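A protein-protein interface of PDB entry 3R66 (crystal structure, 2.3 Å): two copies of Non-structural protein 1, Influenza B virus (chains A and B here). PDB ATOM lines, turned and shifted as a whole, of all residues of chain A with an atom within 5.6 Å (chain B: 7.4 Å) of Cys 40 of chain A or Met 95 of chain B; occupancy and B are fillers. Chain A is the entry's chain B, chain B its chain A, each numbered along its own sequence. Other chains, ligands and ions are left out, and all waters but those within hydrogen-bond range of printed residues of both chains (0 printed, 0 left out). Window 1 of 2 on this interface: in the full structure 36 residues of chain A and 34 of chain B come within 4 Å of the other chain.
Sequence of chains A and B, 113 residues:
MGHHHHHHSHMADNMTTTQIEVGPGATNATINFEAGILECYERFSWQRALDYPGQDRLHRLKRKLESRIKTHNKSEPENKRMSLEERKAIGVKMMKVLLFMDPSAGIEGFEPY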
ATOM      1  N   ALA A  35      16.482  -4.449 -11.857  1.00  0.00           N
ATOM      2  CA  ALA A  35      15.052  -4.576 -12.141  1.00  0.00           C
ATOM      3  C   ALA A  35      14.727  -3.967 -13.510  1.00  0.00           C
ATOM      4  O   ALA A  35      13.948  -4.526 -14.259  1.00  0.00           O
ATOM      5  CB  ALA A  35      14.225  -3.929 -11.037  1.00  0.00           C
ATOM      6  N   GLY A  36      15.346  -2.836 -13.835  1.00  0.00           N
ATOM      7  CA  GLY A  36      15.201  -2.204 -15.152  1.00  0.00           C
ATOM      8  C   GLY A  36      15.728  -3.061 -16.293  1.00  0.00           C
ATOM      9  O   GLY A  36      15.145  -3.104 -17.392  1.00  0.00           O
ATOM     10  N   ILE A  37      16.810  -3.766 -16.016  1.00  0.00           N
ATOM     11  CA  ILE A  37      17.416  -4.665 -16.973  1.00  0.00           C
ATOM     12  C   ILE A  37      16.451  -5.813 -17.277  1.00  0.00           C
ATOM     13  O   ILE A  37      16.285  -6.218 -18.436  1.00  0.00           O
ATOM     14  CB  ILE A  37      18.754  -5.237 -16.430  1.00  0.00           C
ATOM     15  CG1 ILE A  37      19.819  -4.123 -16.324  1.00  0.00           C
ATOM     16  CG2 ILE A  37      19.258  -6.355 -17.326  1.00  0.00           C
ATOM     17  CD1 ILE A  37      20.186  -3.457 -17.642  1.00  0.00           C
ATOM     18  N   LEU A  38      15.811  -6.333 -16.237  1.00  0.00           N
ATOM     19  CA  LEU A  38      14.844  -7.398 -16.402  1.00  0.00           C
ATOM     20  C   LEU A  38      13.691  -6.937 -17.286  1.00  0.00           C
ATOM     21  O   LEU A  38      13.274  -7.648 -18.204  1.00  0.00           O
ATOM     22  CB  LEU A  38      14.299  -7.861 -15.050  1.00  0.00           C
ATOM     23  CG  LEU A  38      13.260  -8.976 -15.103  1.00  0.00           C
ATOM     24  CD1 LEU A  38      13.855 -10.203 -15.793  1.00  0.00           C
ATOM     25  CD2 LEU A  38      12.783  -9.305 -13.712  1.00  0.00           C
ATOM     26  N   GLU A  39      13.163  -5.758 -16.996  1.00  0.00           N
ATOM     27  CA  GLU A  39      12.055  -5.214 -17.764  1.00  0.00           C
ATOM     28  C   GLU A  39      12.396  -5.165 -19.259  1.00  0.00           C
ATOM     29  O   GLU A  39      11.515  -5.349 -20.093  1.00  0.00           O
ATOM     30  CB  GLU A  39      11.696  -3.824 -17.221  1.00  0.00           C
ATOM     31  CG  GLU A  39      10.546  -3.108 -17.915  1.00  0.00           C
ATOM     32  CD  GLU A  39       9.231  -3.879 -17.918  1.00  0.00           C
ATOM     33  OE1 GLU A  39       9.080  -4.893 -17.195  1.00  0.00           O
ATOM     34  OE2 GLU A  39       8.333  -3.463 -18.668  1.00  0.00           O
ATOM     35  N   CYS A  40      13.660  -4.897 -19.587  1.00  0.00           N
ATOM     36  CA  CYS A  40      14.101  -4.824 -20.971  1.00  0.00           C
ATOM     37  C   CYS A  40      14.252  -6.215 -21.563  1.00  0.00           C
ATOM     38  O   CYS A  40      13.904  -6.415 -22.709  1.00  0.00           O
ATOM     39  CB  CYS A  40      15.443  -4.077 -21.103  1.00  0.00           C
ATOM     40  SG  CYS A  40      15.439  -2.344 -20.636  1.00  0.00           S
ATOM     41  N   TYR A  41      14.803  -7.163 -20.800  1.00  0.00           N
ATOM     42  CA  TYR A  41      14.847  -8.553 -21.238  1.00  0.00           C
ATOM     43  C   TYR A  41      13.454  -9.035 -21.594  1.00  0.00           C
ATOM     44  O   TYR A  41      13.241  -9.525 -22.700  1.00  0.00           O
ATOM     45  CB  TYR A  41      15.447  -9.478 -20.168  1.00  0.00           C
ATOM     46  CG  TYR A  41      16.936  -9.707 -20.309  1.00  0.00           C
ATOM     47  CD1 TYR A  41      17.424 -10.766 -21.045  1.00  0.00           C
ATOM     48  CD2 TYR A  41      17.852  -8.859 -19.708  1.00  0.00           C
ATOM     49  CE1 TYR A  41      18.788 -10.987 -21.171  1.00  0.00           C
ATOM     50  CE2 TYR A  41      19.221  -9.076 -19.807  1.00  0.00           C
ATOM     51  CZ  TYR A  41      19.685 -10.128 -20.559  1.00  0.00           C
ATOM     52  OH  TYR A  41      21.045 -10.317 -20.675  1.00  0.00           O
ATOM     53  N   GLU A  42      12.506  -8.823 -20.683  1.00  0.00           N
ATOM     54  CA  GLU A  42      11.102  -9.208 -20.889  1.00  0.00           C
ATOM     55  C   GLU A  42      10.463  -8.563 -22.116  1.00  0.00           C
ATOM     56  O   GLU A  42       9.867  -9.271 -22.930  1.00  0.00           O
ATOM     57  CB  GLU A  42      10.259  -8.891 -19.650  1.00  0.00           C
ATOM     58  CG  GLU A  42      10.596  -9.800 -18.476  1.00  0.00           C
ATOM     59  CD  GLU A  42       9.813  -9.487 -17.223  1.00  0.00           C
ATOM     60  OE1 GLU A  42       9.266  -8.379 -17.114  1.00  0.00           O
ATOM     61  OE2 GLU A  42       9.748 -10.362 -16.345  1.00  0.00           O
ATOM     62  N   ARG A  43      10.611  -7.246 -22.269  1.00  0.00           N
ATOM     63  CA  ARG A  43      10.047  -6.567 -23.427  1.00  0.00           C
ATOM     64  C   ARG A  43      10.694  -7.080 -24.701  1.00  0.00           C
ATOM     65  O   ARG A  43      10.016  -7.285 -25.711  1.00  0.00           O
ATOM     66  CB  ARG A  43      10.241  -5.056 -23.337  1.00  0.00           C
ATOM     67  CG  ARG A  43       9.435  -4.403 -22.241  1.00  0.00           C
ATOM     68  CD  ARG A  43       9.756  -2.915 -22.124  1.00  0.00           C
ATOM     69  NE  ARG A  43       8.943  -2.316 -21.073  1.00  0.00           N
ATOM     70  CZ  ARG A  43       8.814  -1.012 -20.837  1.00  0.00           C
ATOM     71  NH1 ARG A  43       9.435  -0.115 -21.593  1.00  0.00           N
ATOM     72  NH2 ARG A  43       8.052  -0.602 -19.827  1.00  0.00           N
ATOM     73  N   PHE A  44      12.011  -7.261 -24.667  1.00  0.00           N
ATOM     74  CA  PHE A  44      12.731  -7.803 -25.828  1.00  0.00           C
ATOM     75  C   PHE A  44      12.188  -9.184 -26.159  1.00  0.00           C
ATOM     76  O   PHE A  44      11.932  -9.492 -27.323  1.00  0.00           O
ATOM     77  CB  PHE A  44      14.214  -7.864 -25.547  1.00  0.00           C
ATOM     78  CG  PHE A  44      15.063  -8.194 -26.749  1.00  0.00           C
ATOM     79  CD1 PHE A  44      15.039  -7.397 -27.881  1.00  0.00           C
ATOM     80  CD2 PHE A  44      15.918  -9.269 -26.716  1.00  0.00           C
ATOM     81  CE1 PHE A  44      15.836  -7.683 -28.980  1.00  0.00           C
ATOM     82  CE2 PHE A  44      16.712  -9.569 -27.807  1.00  0.00           C
ATOM     83  CZ  PHE A  44      16.677  -8.770 -28.938  1.00  0.00           C
ATOM     84  N   SER A  45      11.900  -9.970 -25.126  1.00  0.00           N
ATOM     85  CA  SER A  45      11.446 -11.327 -25.331  1.00  0.00           C
ATOM     86  C   SER A  45      10.133 -11.404 -26.093  1.00  0.00           C
ATOM     87  O   SER A  45       9.910 -12.338 -26.850  1.00  0.00           O
ATOM     88  CB  SER A  45      11.296 -12.034 -23.998  1.00  0.00           C
ATOM     89  OG  SER A  45      11.044 -13.396 -24.215  1.00  0.00           O
ATOM     90  N   MET A  95      17.739   3.676 -16.729  1.00  0.00           N
ATOM     91  CA  MET A  95      18.215   3.210 -18.035  1.00  0.00           C
ATOM     92  C   MET A  95      18.055   4.272 -19.108  1.00  0.00           C
ATOM     93  O   MET A  95      18.905   4.406 -19.979  1.00  0.00           O
ATOM     94  CB  MET A  95      17.404   2.016 -18.506  1.00  0.00           C
ATOM     95  CG  MET A  95      18.207   0.938 -19.183  1.00  0.00           C
ATOM     96  SD  MET A  95      19.119   0.079 -17.899  1.00  0.00           S
ATOM     97  CE  MET A  95      17.757  -1.032 -17.527  1.00  0.00           C
ATOM     98  N   LEU A  99      21.043   5.613 -21.203  1.00  0.00           N
ATOM     99  CA  LEU A  99      21.060   5.426 -22.659  1.00  0.00           C
ATOM    100  C   LEU A  99      21.247   6.753 -23.425  1.00  0.00           C
ATOM    101  O   LEU A  99      21.934   6.782 -24.451  1.00  0.00           O
ATOM    102  CB  LEU A  99      19.808   4.682 -23.127  1.00  0.00           C
ATOM    103  CG  LEU A  99      19.728   3.192 -22.826  1.00  0.00           C
ATOM    104  CD1 LEU A  99      18.259   2.790 -22.748  1.00  0.00           C
ATOM    105  CD2 LEU A  99      20.473   2.399 -23.895  1.00  0.00           C
ATOM    106  N   ASN B  32      23.454  -8.679 -29.825  1.00  0.00           N
ATOM    107  CA  ASN B  32      23.380  -7.223 -29.938  1.00  0.00           C
ATOM    108  C   ASN B  32      22.622  -6.586 -28.784  1.00  0.00           C
ATOM    109  O   ASN B  32      23.123  -5.677 -28.139  1.00  0.00           O
ATOM    110  CB  ASN B  32      22.796  -6.825 -31.289  1.00  0.00           C
ATOM    111  CG  ASN B  32      23.662  -7.302 -32.427  1.00  0.00           C
ATOM    112  OD1 ASN B  32      24.832  -7.606 -32.223  1.00  0.00           O
ATOM    113  ND2 ASN B  32      23.091  -7.428 -33.609  1.00  0.00           N
ATOM    114  N   PHE B  33      21.441  -7.091 -28.498  1.00  0.00           N
ATOM    115  CA  PHE B  33      20.710  -6.666 -27.305  1.00  0.00           C
ATOM    116  C   PHE B  33      21.593  -6.760 -26.062  1.00  0.00           C
ATOM    117  O   PHE B  33      21.715  -5.803 -25.304  1.00  0.00           O
ATOM    118  CB  PHE B  33      19.480  -7.537 -27.112  1.00  0.00           C
ATOM    119  CG  PHE B  33      18.737  -7.251 -25.849  1.00  0.00           C
ATOM    120  CD1 PHE B  33      17.967  -6.104 -25.721  1.00  0.00           C
ATOM    121  CD2 PHE B  33      18.796  -8.132 -24.783  1.00  0.00           C
ATOM    122  CE1 PHE B  33      17.267  -5.843 -24.554  1.00  0.00           C
ATOM    123  CE2 PHE B  33      18.104  -7.878 -23.603  1.00  0.00           C
ATOM    124  CZ  PHE B  33      17.358  -6.725 -23.486  1.00  0.00           C
ATOM    125  N   GLU B  34      22.229  -7.912 -25.858  1.00  0.00           N
ATOM    126  CA  GLU B  34      23.028  -8.102 -24.647  1.00  0.00           C
ATOM    127  C   GLU B  34      24.308  -7.281 -24.645  1.00  0.00           C
ATOM    128  O   GLU B  34      24.787  -6.920 -23.582  1.00  0.00           O
ATOM    129  CB  GLU B  34      23.296  -9.568 -24.397  1.00  0.00           C
ATOM    130  CG  GLU B  34      22.078 -10.222 -23.761  1.00  0.00           C
ATOM    131  CD  GLU B  34      22.318 -11.644 -23.381  1.00  0.00           C
ATOM    132  OE1 GLU B  34      22.924 -12.376 -24.183  1.00  0.00           O
ATOM    133  OE2 GLU B  34      21.870 -12.037 -22.292  1.00  0.00           O
ATOM    134  N   ALA B  35      24.837  -6.956 -25.824  1.00  0.00           N
ATOM    135  CA  ALA B  35      25.876  -5.922 -25.920  1.00  0.00           C
ATOM    136  C   ALA B  35      25.341  -4.582 -25.411  1.00  0.00           C
ATOM    137  O   ALA B  35      26.044  -3.875 -24.713  1.00  0.00           O
ATOM    138  CB  ALA B  35      26.391  -5.776 -27.336  1.00  0.00           C
ATOM    139  N   GLY B  36      24.095  -4.254 -25.735  1.00  0.00           N
ATOM    140  CA  GLY B  36      23.436  -3.046 -25.211  1.00  0.00           C
ATOM    141  C   GLY B  36      23.315  -3.043 -23.690  1.00  0.00           C
ATOM    142  O   GLY B  36      23.466  -2.007 -23.032  1.00  0.00           O
ATOM    143  N   ILE B  37      23.034  -4.201 -23.142  1.00  0.00           N
ATOM    144  CA  ILE B  37      22.876  -4.390 -21.699  1.00  0.00           C
ATOM    145  C   ILE B  37      24.212  -4.139 -21.002  1.00  0.00           C
ATOM    146  O   ILE B  37      24.273  -3.494 -19.958  1.00  0.00           O
ATOM    147  CB  ILE B  37      22.388  -5.838 -21.392  1.00  0.00           C
ATOM    148  CG1 ILE B  37      20.964  -6.054 -21.913  1.00  0.00           C
ATOM    149  CG2 ILE B  37      22.465  -6.178 -19.910  1.00  0.00           C
ATOM    150  CD1 ILE B  37      19.934  -5.139 -21.296  1.00  0.00           C
ATOM    151  N   LEU B  38      25.288  -4.608 -21.616  1.00  0.00           N
ATOM    152  CA  LEU B  38      26.620  -4.387 -21.080  1.00  0.00           C
ATOM    153  C   LEU B  38      26.950  -2.895 -21.045  1.00  0.00           C
ATOM    154  O   LEU B  38      27.439  -2.389 -20.042  1.00  0.00           O
ATOM    155  CB  LEU B  38      27.664  -5.119 -21.919  1.00  0.00           C
ATOM    156  CG  LEU B  38      29.112  -4.950 -21.479  1.00  0.00           C
ATOM    157  CD1 LEU B  38      29.289  -5.458 -20.050  1.00  0.00           C
ATOM    158  CD2 LEU B  38      30.015  -5.703 -22.452  1.00  0.00           C
ATOM    159  N   GLU B  39      26.671  -2.206 -22.146  1.00  0.00           N
ATOM    160  CA  GLU B  39      26.915  -0.789 -22.242  1.00  0.00           C
ATOM    161  C   GLU B  39      26.209  -0.021 -21.123  1.00  0.00           C
ATOM    162  O   GLU B  39      26.742   0.953 -20.610  1.00  0.00           O
ATOM    163  CB  GLU B  39      26.460  -0.285 -23.613  1.00  0.00           C
ATOM    164  CG  GLU B  39      26.657   1.197 -23.860  1.00  0.00           C
ATOM    165  CD  GLU B  39      28.088   1.676 -23.702  1.00  0.00           C
ATOM    166  OE1 GLU B  39      29.029   0.853 -23.650  1.00  0.00           O
ATOM    167  OE2 GLU B  39      28.269   2.909 -23.656  1.00  0.00           O
ATOM    168  N   CYS B  40      25.022  -0.480 -20.727  1.00  0.00           N
ATOM    169  CA  CYS B  40      24.281   0.145 -19.630  1.00  0.00           C
ATOM    170  C   CYS B  40      24.895  -0.226 -18.264  1.00  0.00           C
ATOM    171  O   CYS B  40      24.963   0.618 -17.384  1.00  0.00           O
ATOM    172  CB  CYS B  40      22.811  -0.262 -19.675  1.00  0.00           C
ATOM    173  SG  CYS B  40      21.919   0.301 -21.171  1.00  0.00           S
ATOM    174  N   TYR B  41      25.296  -1.487 -18.068  1.00  0.00           N
ATOM    175  CA  TYR B  41      26.043  -1.861 -16.845  1.00  0.00           C
ATOM    176  C   TYR B  41      27.240  -0.957 -16.679  1.00  0.00           C
ATOM    177  O   TYR B  41      27.408  -0.328 -15.643  1.00  0.00           O
ATOM    178  CB  TYR B  41      26.461  -3.333 -16.839  1.00  0.00           C
ATOM    179  CG  TYR B  41      25.470  -4.277 -16.162  1.00  0.00           C
ATOM    180  CD1 TYR B  41      25.594  -4.626 -14.826  1.00  0.00           C
ATOM    181  CD2 TYR B  41      24.434  -4.855 -16.889  1.00  0.00           C
ATOM    182  CE1 TYR B  41      24.703  -5.521 -14.221  1.00  0.00           C
ATOM    183  CE2 TYR B  41      23.524  -5.731 -16.296  1.00  0.00           C
ATOM    184  CZ  TYR B  41      23.652  -6.056 -14.965  1.00  0.00           C
ATOM    185  OH  TYR B  41      22.759  -6.947 -14.408  1.00  0.00           O
ATOM    186  N   ALA B  89      26.225  -0.244 -30.138  1.00  0.00           N
ATOM    187  CA  ALA B  89      25.393   0.828 -30.707  1.00  0.00           C
ATOM    188  C   ALA B  89      24.029   0.329 -31.195  1.00  0.00           C
ATOM    189  O   ALA B  89      23.027   1.046 -31.084  1.00  0.00           O
ATOM    190  CB  ALA B  89      26.127   1.526 -31.850  1.00  0.00           C
ATOM    191  N   ILE B  90      24.006  -0.888 -31.746  1.00  0.00           N
ATOM    192  CA  ILE B  90      22.761  -1.510 -32.218  1.00  0.00           C
ATOM    193  C   ILE B  90      21.885  -1.882 -31.023  1.00  0.00           C
ATOM    194  O   ILE B  90      20.674  -1.644 -31.042  1.00  0.00           O
ATOM    195  CB  ILE B  90      23.031  -2.760 -33.089  1.00  0.00           C
ATOM    196  CG1 ILE B  90      23.722  -2.364 -34.404  1.00  0.00           C
ATOM    197  CG2 ILE B  90      21.736  -3.481 -33.409  1.00  0.00           C
ATOM    198  CD1 ILE B  90      24.505  -3.481 -35.072  1.00  0.00           C
ATOM    199  N   GLY B  91      22.495  -2.446 -29.979  1.00  0.00           N
ATOM    200  CA  GLY B  91      21.771  -2.808 -28.762  1.00  0.00           C
ATOM    201  C   GLY B  91      21.174  -1.619 -28.024  1.00  0.00           C
ATOM    202  O   GLY B  91      20.098  -1.714 -27.469  1.00  0.00           O
ATOM    203  N   VAL B  92      21.911  -0.513 -27.977  1.00  0.00           N
ATOM    204  CA  VAL B  92      21.442   0.718 -27.344  1.00  0.00           C
ATOM    205  C   VAL B  92      20.165   1.239 -28.032  1.00  0.00           C
ATOM    206  O   VAL B  92      19.169   1.543 -27.369  1.00  0.00           O
ATOM    207  CB  VAL B  92      22.547   1.808 -27.365  1.00  0.00           C
ATOM    208  CG1 VAL B  92      21.931   3.200 -27.288  1.00  0.00           C
ATOM    209  CG2 VAL B  92      23.550   1.578 -26.241  1.00  0.00           C
ATOM    210  N   LYS B  93      20.192   1.311 -29.355  1.00  0.00           N
ATOM    211  CA  LYS B  93      18.991   1.676 -30.136  1.00  0.00           C
ATOM    212  C   LYS B  93      17.824   0.743 -29.851  1.00  0.00           C
ATOM    213  O   LYS B  93      16.691   1.206 -29.660  1.00  0.00           O
ATOM    214  CB  LYS B  93      19.307   1.665 -31.627  1.00  0.00           C
ATOM    215  CG  LYS B  93      20.251   2.780 -32.034  1.00  0.00           C
ATOM    216  CD  LYS B  93      20.658   2.673 -33.492  1.00  0.00           C
ATOM    217  CE  LYS B  93      21.867   3.557 -33.800  1.00  0.00           C
ATOM    218  NZ  LYS B  93      22.335   3.394 -35.200  1.00  0.00           N
ATOM    219  N   MET B  94      18.096  -0.567 -29.808  1.00  0.00           N
ATOM    220  CA  MET B  94      17.055  -1.555 -29.502  1.00  0.00           C
ATOM    221  C   MET B  94      16.449  -1.266 -28.142  1.00  0.00           C
ATOM    222  O   MET B  94      15.224  -1.289 -27.975  1.00  0.00           O
ATOM    223  CB  MET B  94      17.603  -2.989 -29.519  1.00  0.00           C
ATOM    224  CG  MET B  94      17.682  -3.642 -30.888  1.00  0.00           C
ATOM    225  SD  MET B  94      18.473  -5.270 -30.793  1.00  0.00           S
ATOM    226  CE  MET B  94      18.136  -5.805 -32.457  1.00  0.00           C
ATOM    227  N   MET B  95      17.314  -0.997 -27.172  1.00  0.00           N
ATOM    228  CA  MET B  95      16.876  -0.729 -25.804  1.00  0.00           C
ATOM    229  C   MET B  95      16.098   0.580 -25.696  1.00  0.00           C
ATOM    230  O   MET B  95      15.112   0.661 -24.943  1.00  0.00           O
ATOM    231  CB  MET B  95      18.073  -0.776 -24.848  1.00  0.00           C
ATOM    232  CG  MET B  95      18.257  -2.116 -24.174  1.00  0.00           C
ATOM    233  SD  MET B  95      19.737  -1.999 -23.156  1.00  0.00           S
ATOM    234  CE  MET B  95      18.978  -1.474 -21.605  1.00  0.00           C
ATOM    235  N   LYS B  96      16.509   1.593 -26.465  1.00  0.00           N
ATOM    236  CA  LYS B  96      15.747   2.850 -26.536  1.00  0.00           C
ATOM    237  C   LYS B  96      14.328   2.603 -27.082  1.00  0.00           C
ATOM    238  O   LYS B  96      13.345   3.049 -26.495  1.00  0.00           O
ATOM    239  CB  LYS B  96      16.473   3.899 -27.394  1.00  0.00           C
ATOM    240  CG  LYS B  96      17.757   4.457 -26.765  1.00  0.00           C
ATOM    241  CD  LYS B  96      18.517   5.333 -27.747  1.00  0.00           C
ATOM    242  CE  LYS B  96      19.722   6.020 -27.112  1.00  0.00           C
ATOM    243  NZ  LYS B  96      20.588   6.665 -28.139  1.00  0.00           N
ATOM    244  N   VAL B  97      14.231   1.862 -28.179  1.00  0.00           N
ATOM    245  CA  VAL B  97      12.918   1.521 -28.748  1.00  0.00           C
ATOM    246  C   VAL B  97      12.015   0.830 -27.722  1.00  0.00           C
ATOM    247  O   VAL B  97      10.835   1.134 -27.634  1.00  0.00           O
ATOM    248  CB  VAL B  97      13.033   0.631 -30.008  1.00  0.00           C
ATOM    249  CG1 VAL B  97      11.689   0.021 -30.387  1.00  0.00           C
ATOM    250  CG2 VAL B  97      13.576   1.424 -31.171  1.00  0.00           C
ATOM    251  N   LEU B  98      12.574  -0.090 -26.947  1.00  0.00           N
ATOM    252  CA  LEU B  98      11.769  -0.853 -25.994  1.00  0.00           C
ATOM    253  C   LEU B  98      11.425  -0.013 -24.764  1.00  0.00           C
ATOM    254  O   LEU B  98      10.309  -0.034 -24.289  1.00  0.00           O
ATOM    255  CB  LEU B  98      12.519  -2.121 -25.564  1.00  0.00           C
ATOM    256  CG  LEU B  98      12.829  -3.193 -26.614  1.00  0.00           C
ATOM    257  CD1 LEU B  98      14.057  -4.004 -26.195  1.00  0.00           C
ATOM    258  CD2 LEU B  98      11.635  -4.098 -26.830  1.00  0.00           C
ATOM    259  N   LEU B  99      12.390   0.721 -24.230  1.00  0.00           N
ATOM    260  CA  LEU B  99      12.120   1.519 -23.033  1.00  0.00           C
ATOM    261  C   LEU B  99      11.033   2.577 -23.269  1.00  0.00           C
ATOM    262  O   LEU B  99      10.233   2.850 -22.373  1.00  0.00           O
ATOM    263  CB  LEU B  99      13.411   2.145 -22.489  1.00  0.00           C
ATOM    264  CG  LEU B  99      14.189   1.077 -21.697  1.00  0.00           C
ATOM    265  CD1 LEU B  99      15.408   1.640 -21.038  1.00  0.00           C
ATOM    266  CD2 LEU B  99      13.351   0.356 -20.646  1.00  0.00           C
ATOM    267  N   PHE B 100      10.983   3.143 -24.473  1.00  0.00           N
ATOM    268  CA  PHE B 100       9.949   4.103 -24.809  1.00  0.00           C
ATOM    269  C   PHE B 100       8.773   3.507 -25.545  1.00  0.00           C
ATOM    270  O   PHE B 100       7.761   4.189 -25.714  1.00  0.00           O
ATOM    271  CB  PHE B 100      10.543   5.252 -25.622  1.00  0.00           C
ATOM    272  CG  PHE B 100      11.434   6.133 -24.802  1.00  0.00           C
ATOM    273  CD1 PHE B 100      10.922   7.254 -24.160  1.00  0.00           C
ATOM    274  CD2 PHE B 100      12.762   5.807 -24.619  1.00  0.00           C
ATOM    275  CE1 PHE B 100      11.731   8.061 -23.382  1.00  0.00           C
ATOM    276  CE2 PHE B 100      13.571   6.603 -23.829  1.00  0.00           C
ATOM    277  CZ  PHE B 100      13.056   7.747 -23.220  1.00  0.00           C
ATOM    278  N   MET B 101       8.890   2.243 -25.956  1.00  0.00           N
ATOM    279  CA  MET B 101       7.882   1.598 -26.791  1.00  0.00           C
ATOM    280  C   MET B 101       7.575   2.524 -27.957  1.00  0.00           C
ATOM    281  O   MET B 101       6.447   2.979 -28.134  1.00  0.00           O
ATOM    282  CB  MET B 101       6.626   1.257 -25.979  1.00  0.00           C
ATOM    283  CG  MET B 101       6.787   0.008 -25.122  1.00  0.00           C
ATOM    284  SD  MET B 101       6.853  -1.515 -26.078  1.00  0.00           S
ATOM    285  CE  MET B 101       7.919  -2.487 -25.022  1.00  0.00           C
ATOM    286  N   ALA B 105      12.680   5.909 -31.561  1.00  0.00           N
ATOM    287  CA  ALA B 105      13.783   6.031 -30.577  1.00  0.00           C
ATOM    288  C   ALA B 105      15.251   5.869 -31.033  1.00  0.00           C
ATOM    289  O   ALA B 105      16.086   6.586 -30.510  1.00  0.00           O
ATOM    290  CB  ALA B 105      13.509   5.143 -29.382  1.00  0.00           C
ATOM    291  N   GLY B 106      15.643   4.925 -31.891  1.00  0.00           N
ATOM    292  CA  GLY B 106      14.901   3.764 -32.242  1.00  0.00           C
ATOM    293  C   GLY B 106      15.162   3.110 -33.600  1.00  0.00           C
ATOM    294  O   GLY B 106      15.621   1.960 -33.671  1.00  0.00           O
ATOM    295  N   GLY B 109      17.247  -0.064 -34.867  1.00  0.00           N
ATOM    296  CA  GLY B 109      17.106  -1.357 -34.166  1.00  0.00           C
ATOM    297  C   GLY B 109      16.322  -2.408 -34.958  1.00  0.00           C
ATOM    298  O   GLY B 109      16.413  -3.606 -34.666  1.00  0.00           O
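Cys 40 of chain A touches Met 95 of chain B, but with the chains exchanged Met 95 of chain A does not touch Cys 40 of chain B (4.1 Å).
Cys 40 of chain A touches Leu 99 of chain B, and with the chains exchanged Leu 99 of chain A touches Cys 40 of chain B.
Met 95 of chain A touches its own counterpart, Met 95 of chain B.
Leu 99 of chain B touches its own counterpart, Leu 99 of chain A.
Positions printed for both chains: 35, 36, 37, 38, 39, 40, 41, 95 and 99.
Cys 40 of chain A touches just these residues of chain B: Phe 33 (3.6 Å), Met 95 (3.8 Å) and Leu 99 (3.4 Å).
Met 95 of chain B touches two residues of chain A.
Of the printed residues of chain A, Leu 99 of chain B touches Cys 40, Arg 43, Met 95 and Leu 99.
Of the printed residues of chain B, Arg 43 of chain A touches Leu 98 (2.8 Å), Leu 99 (3.2 Å) and Met 101 (3.5 Å).
Of the printed residues of chain A, Lys 96 of chain B touches Leu 99.
Leu 38 of chain A touches none of the printed residues of chain B.
Ala 35 of chain A touches none of the printed residues of chain B.
SG of Cys 40 of chain A sits at hydrogen-bond distance from O of Gly 36 of chain A, 3.3 Å away.
The backbone carbonyl oxygen of Gly 36 of chain B is in hydrogen-bond range of the side-chain sulfur of Cys 40 of chain B (3.3 Å).
OE2 of Glu 39 of chain A lies within salt-bridge range of NE of Arg 43 of chain A (2.7 Å).
The side-chain sulfur (SG) of Cys 40 of chain B sits close to the side-chain sulfur (SD) of Met 95 of chain B, at 3.7 Å.
Among the printed residues, pairs that only touch across the chains: Cys 40 of chain A with Phe 33 of chain B (3.6 Å), Cys 40 of chain A with Met 95 of chain B (3.8 Å), Cys 40 of chain A with Leu 99 of chain B (3.4 Å), Tyr 41 of chain A with Phe 33 of chain B (3.7 Å), Arg 43 of chain A with Met 101 of chain B (3.5 Å), Phe 44 of chain A with Phe 33 of chain B (3.5 Å), Phe 44 of chain A with Leu 98 of chain B (3.9 Å), Met 95 of chain A with Met 95 of chain B (3.5 Å), Met 95 of chain A with Leu 99 of chain B (3.2 Å), Leu 99 of chain A with Cys 40 of chain B (3.7 Å), Leu 99 of chain A with Val 92 of chain B (3.8 Å), Leu 99 of chain A with Lys 96 of chain B (3.5 Å) and Leu 99 of chain A with Leu 99 of chain B (3.5 Å).
O of Leu 99 of chain B lies within hydrogen-bond range of NH1 of Arg 43 of chain A (3.2 Å).
The guanidinium group (NH1) of Arg 43 of chain A sits at hydrogen-bond distance from the backbone carbonyl oxygen (O) of Leu 98 of chain B (2.8 Å).
The side-chain carboxylate (OE2) of Glu 34 of chain B sits at hydrogen-bond distance from the side-chain hydroxyl (OH) of Tyr 41 of chain A, at 2.5 Å.
Printed residues of chain B that touch a printed residue of chain A: Phe 33, Glu 34, Cys 40, Val 92, Met 95, Lys 96, Leu 98, Leu 99 and Met 101.
Of the 13 printed residues of chain A, 6 touch a printed residue of chain B.
Printed residues of chain A that touch a printed residue of chain B: Cys 40, Tyr 41, Arg 43, Phe 44, Met 95 and Leu 99.
Hydrophobic or aromatic side chains of chain A that line the printed part of chain B: Tyr 41, Phe 44, Met 95 and Leu 99.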
